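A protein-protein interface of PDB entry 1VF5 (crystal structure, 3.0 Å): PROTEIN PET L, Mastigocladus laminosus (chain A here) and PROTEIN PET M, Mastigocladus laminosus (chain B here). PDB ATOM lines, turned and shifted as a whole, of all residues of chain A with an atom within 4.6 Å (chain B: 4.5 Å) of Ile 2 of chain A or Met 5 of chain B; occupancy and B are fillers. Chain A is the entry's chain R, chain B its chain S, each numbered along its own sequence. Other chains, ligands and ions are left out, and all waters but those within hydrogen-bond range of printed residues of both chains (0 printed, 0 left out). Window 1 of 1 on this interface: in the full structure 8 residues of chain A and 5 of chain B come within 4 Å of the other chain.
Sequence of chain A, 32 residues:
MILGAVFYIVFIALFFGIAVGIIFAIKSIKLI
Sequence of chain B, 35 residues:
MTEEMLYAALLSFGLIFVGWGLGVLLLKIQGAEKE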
ATOM      1  N   MET A   1       5.395 -23.226   0.542  1.00  0.00           N
ATOM      2  CA  MET A   1       6.750 -22.746   0.202  1.00  0.00           C
ATOM      3  C   MET A   1       6.750 -21.280  -0.200  1.00  0.00           C
ATOM      4  O   MET A   1       5.709 -20.624  -0.299  1.00  0.00           O
ATOM      5  CB  MET A   1       7.360 -23.605  -0.913  1.00  0.00           C
ATOM      6  CG  MET A   1       7.659 -25.057  -0.505  1.00  0.00           C
ATOM      7  SD  MET A   1       6.266 -26.281  -0.356  1.00  0.00           S
ATOM      8  CE  MET A   1       5.602 -25.998   1.312  1.00  0.00           C
ATOM      9  N   ILE A   2       7.948 -20.769  -0.421  1.00  0.00           N
ATOM     10  CA  ILE A   2       8.134 -19.384  -0.799  1.00  0.00           C
ATOM     11  C   ILE A   2       7.483 -19.050  -2.132  1.00  0.00           C
ATOM     12  O   ILE A   2       6.635 -18.160  -2.208  1.00  0.00           O
ATOM     13  CB  ILE A   2       9.647 -19.059  -0.872  1.00  0.00           C
ATOM     14  CG1 ILE A   2       9.883 -17.823  -1.749  1.00  0.00           C
ATOM     15  CG2 ILE A   2      10.418 -20.287  -1.381  1.00  0.00           C
ATOM     16  CD1 ILE A   2       9.154 -16.577  -1.282  1.00  0.00           C
ATOM     17  N   LEU A   3       7.896 -19.768  -3.176  1.00  0.00           N
ATOM     18  CA  LEU A   3       7.372 -19.550  -4.515  1.00  0.00           C
ATOM     19  C   LEU A   3       5.887 -19.792  -4.456  1.00  0.00           C
ATOM     20  O   LEU A   3       5.143 -19.359  -5.333  1.00  0.00           O
ATOM     21  CB  LEU A   3       8.005 -20.507  -5.543  1.00  0.00           C
ATOM     22  CG  LEU A   3       7.471 -21.940  -5.673  1.00  0.00           C
ATOM     23  CD1 LEU A   3       8.008 -22.593  -6.921  1.00  0.00           C
ATOM     24  CD2 LEU A   3       7.859 -22.742  -4.447  1.00  0.00           C
ATOM     25  N   GLY A   4       5.459 -20.502  -3.417  1.00  0.00           N
ATOM     26  CA  GLY A   4       4.057 -20.771  -3.278  1.00  0.00           C
ATOM     27  C   GLY A   4       3.328 -19.517  -3.642  1.00  0.00           C
ATOM     28  O   GLY A   4       2.417 -19.543  -4.440  1.00  0.00           O
ATOM     29  N   ALA A   5       3.770 -18.400  -3.086  1.00  0.00           N
ATOM     30  CA  ALA A   5       3.140 -17.117  -3.362  1.00  0.00           C
ATOM     31  C   ALA A   5       3.765 -16.324  -4.490  1.00  0.00           C
ATOM     32  O   ALA A   5       3.170 -15.363  -4.965  1.00  0.00           O
ATOM     33  CB  ALA A   5       3.132 -16.284  -2.122  1.00  0.00           C
ATOM     34  N   VAL A   6       4.975 -16.689  -4.893  1.00  0.00           N
ATOM     35  CA  VAL A   6       5.628 -15.977  -5.984  1.00  0.00           C
ATOM     36  C   VAL A   6       4.737 -16.052  -7.209  1.00  0.00           C
ATOM     37  O   VAL A   6       4.548 -15.060  -7.901  1.00  0.00           O
ATOM     38  CB  VAL A   6       6.997 -16.587  -6.353  1.00  0.00           C
ATOM     39  CG1 VAL A   6       7.549 -15.911  -7.581  1.00  0.00           C
ATOM     40  CG2 VAL A   6       7.961 -16.426  -5.199  1.00  0.00           C
ATOM     41  N   TYR A   8       1.490 -17.420  -7.037  1.00  0.00           N
ATOM     42  CA  TYR A   8       0.085 -17.310  -6.645  1.00  0.00           C
ATOM     43  C   TYR A   8      -0.402 -15.913  -7.009  1.00  0.00           C
ATOM     44  O   TYR A   8      -1.582 -15.705  -7.260  1.00  0.00           O
ATOM     45  CB  TYR A   8      -0.093 -17.539  -5.133  1.00  0.00           C
ATOM     46  CG  TYR A   8      -0.424 -18.978  -4.710  1.00  0.00           C
ATOM     47  CD1 TYR A   8      -0.281 -19.385  -3.375  1.00  0.00           C
ATOM     48  CD2 TYR A   8      -0.875 -19.932  -5.637  1.00  0.00           C
ATOM     49  CE1 TYR A   8      -0.577 -20.706  -2.977  1.00  0.00           C
ATOM     50  CE2 TYR A   8      -1.172 -21.256  -5.245  1.00  0.00           C
ATOM     51  CZ  TYR A   8      -1.018 -21.630  -3.920  1.00  0.00           C
ATOM     52  OH  TYR A   8      -1.302 -22.924  -3.543  1.00  0.00           O
ATOM     53  N   THR B   2       2.588 -19.404   6.447  1.00  0.00           N
ATOM     54  CA  THR B   2       1.978 -18.769   5.277  1.00  0.00           C
ATOM     55  C   THR B   2       2.519 -17.351   5.054  1.00  0.00           C
ATOM     56  O   THR B   2       2.832 -16.972   3.927  1.00  0.00           O
ATOM     57  CB  THR B   2       0.417 -18.703   5.411  1.00  0.00           C
ATOM     58  OG1 THR B   2      -0.152 -18.146   4.217  1.00  0.00           O
ATOM     59  CG2 THR B   2       0.002 -17.843   6.610  1.00  0.00           C
ATOM     60  N   GLU B   3       2.645 -16.586   6.137  1.00  0.00           N
ATOM     61  CA  GLU B   3       3.123 -15.205   6.082  1.00  0.00           C
ATOM     62  C   GLU B   3       4.460 -14.989   5.347  1.00  0.00           C
ATOM     63  O   GLU B   3       4.860 -13.845   5.082  1.00  0.00           O
ATOM     64  CB  GLU B   3       3.186 -14.625   7.512  1.00  0.00           C
ATOM     65  CG  GLU B   3       1.799 -14.387   8.161  1.00  0.00           C
ATOM     66  CD  GLU B   3       1.863 -13.818   9.584  1.00  0.00           C
ATOM     67  OE1 GLU B   3       2.283 -14.555  10.508  1.00  0.00           O
ATOM     68  OE2 GLU B   3       1.489 -12.635   9.776  1.00  0.00           O
ATOM     69  N   GLU B   4       5.143 -16.081   5.009  1.00  0.00           N
ATOM     70  CA  GLU B   4       6.416 -15.996   4.291  1.00  0.00           C
ATOM     71  C   GLU B   4       6.169 -15.821   2.793  1.00  0.00           C
ATOM     72  O   GLU B   4       6.987 -15.247   2.071  1.00  0.00           O
ATOM     73  CB  GLU B   4       7.235 -17.262   4.528  1.00  0.00           C
ATOM     74  CG  GLU B   4       7.653 -17.454   5.970  1.00  0.00           C
ATOM     75  CD  GLU B   4       8.353 -18.774   6.194  1.00  0.00           C
ATOM     76  OE1 GLU B   4       9.234 -19.121   5.377  1.00  0.00           O
ATOM     77  OE2 GLU B   4       8.026 -19.459   7.186  1.00  0.00           O
ATOM     78  N   MET B   5       5.027 -16.334   2.342  1.00  0.00           N
ATOM     79  CA  MET B   5       4.638 -16.246   0.953  1.00  0.00           C
ATOM     80  C   MET B   5       3.670 -15.078   0.819  1.00  0.00           C
ATOM     81  O   MET B   5       3.669 -14.379  -0.187  1.00  0.00           O
ATOM     82  CB  MET B   5       3.956 -17.540   0.511  1.00  0.00           C
ATOM     83  CG  MET B   5       2.499 -17.642   0.941  1.00  0.00           C
ATOM     84  SD  MET B   5       1.615 -18.971   0.100  1.00  0.00           S
ATOM     85  CE  MET B   5       2.151 -20.397   1.067  1.00  0.00           C
ATOM     86  N   LEU B   6       2.849 -14.864   1.845  1.00  0.00           N
ATOM     87  CA  LEU B   6       1.874 -13.771   1.838  1.00  0.00           C
ATOM     88  C   LEU B   6       2.548 -12.446   1.518  1.00  0.00           C
ATOM     89  O   LEU B   6       1.960 -11.586   0.870  1.00  0.00           O
ATOM     90  CB  LEU B   6       1.148 -13.673   3.189  1.00  0.00           C
ATOM     91  CG  LEU B   6       0.295 -14.877   3.621  1.00  0.00           C
ATOM     92  CD1 LEU B   6      -0.264 -14.629   5.013  1.00  0.00           C
ATOM     93  CD2 LEU B   6      -0.839 -15.118   2.623  1.00  0.00           C
ATOM     94  N   TYR B   7       3.780 -12.274   1.981  1.00  0.00           N
ATOM     95  CA  TYR B   7       4.504 -11.051   1.684  1.00  0.00           C
ATOM     96  C   TYR B   7       5.262 -11.309   0.377  1.00  0.00           C
ATOM     97  O   TYR B   7       5.471 -10.403  -0.430  1.00  0.00           O
ATOM     98  CB  TYR B   7       5.448 -10.669   2.855  1.00  0.00           C
ATOM     99  CG  TYR B   7       6.851 -11.272   2.881  1.00  0.00           C
ATOM    100  CD1 TYR B   7       7.751 -11.057   1.834  1.00  0.00           C
ATOM    101  CD2 TYR B   7       7.307 -11.985   3.995  1.00  0.00           C
ATOM    102  CE1 TYR B   7       9.073 -11.531   1.890  1.00  0.00           C
ATOM    103  CE2 TYR B   7       8.633 -12.464   4.065  1.00  0.00           C
ATOM    104  CZ  TYR B   7       9.509 -12.230   3.006  1.00  0.00           C
ATOM    105  OH  TYR B   7      10.816 -12.677   3.059  1.00  0.00           O
ATOM    106  N   ALA B   8       5.633 -12.571   0.169  1.00  0.00           N
ATOM    107  CA  ALA B   8       6.354 -12.990  -1.029  1.00  0.00           C
ATOM    108  C   ALA B   8       5.524 -12.775  -2.289  1.00  0.00           C
ATOM    109  O   ALA B   8       6.066 -12.521  -3.363  1.00  0.00           O
ATOM    110  CB  ALA B   8       6.729 -14.445  -0.912  1.00  0.00           C
ATOM    111  N   ALA B   9       4.209 -12.892  -2.152  1.00  0.00           N
ATOM    112  CA  ALA B   9       3.295 -12.703  -3.269  1.00  0.00           C
ATOM    113  C   ALA B   9       2.990 -11.223  -3.500  1.00  0.00           C
ATOM    114  O   ALA B   9       3.020 -10.750  -4.625  1.00  0.00           O
ATOM    115  CB  ALA B   9       2.007 -13.460  -3.017  1.00  0.00           C
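Among the printed residues, pairs that only touch across the chains: Met 1 of chain A with Met 5 of chain B (3.6 Å), Ile 2 of chain A with Met 5 of chain B (3.9 Å), Ile 2 of chain A with Ala 8 of chain B (3.3 Å), Ala 5 of chain A with Met 5 of chain B (2.8 Å), Ala 5 of chain A with Ala 9 of chain B (3.0 Å) and Tyr 8 of chain A with Met 5 of chain B (3.98 Å).
Of the printed residues of chain B, Met 1 of chain A touches Met 5 (3.6 Å). Of chain B, only Met 5 (3.9 Å) and Ala 8 (3.3 Å) come within 4 Å of Ile 2 of chain A. Glu 3 of chain B touches none of the printed residues of chain A. Of the printed residues of chain A, Met 5 of chain B touches Met 1, Ile 2, Ala 5 and Tyr 8. Of the printed residues of chain A, Ala 9 of chain B touches Ala 5. The nearest printed residue of chain A that does not touch Met 5 of chain B is Gly 4 of chain A (4.2 Å). The nearest printed residue of chain B that does not touch Met 1 of chain A is Glu 4 of chain B (5.7 Å).
Of the 8 printed residues of chain B, 3 touch a printed residue of chain A. Hydrophobic or aromatic side chains of chain B within 4 Å of the printed part of chain A: Met 5, Ala 8 and Ala 9. Of the 7 printed residues of chain A, 4 touch a printed residue of chain B. Hydrophobic or aromatic side chains of chain A within 4 Å of the printed part of chain B: Ile 2, Ala 5 and Tyr 8.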
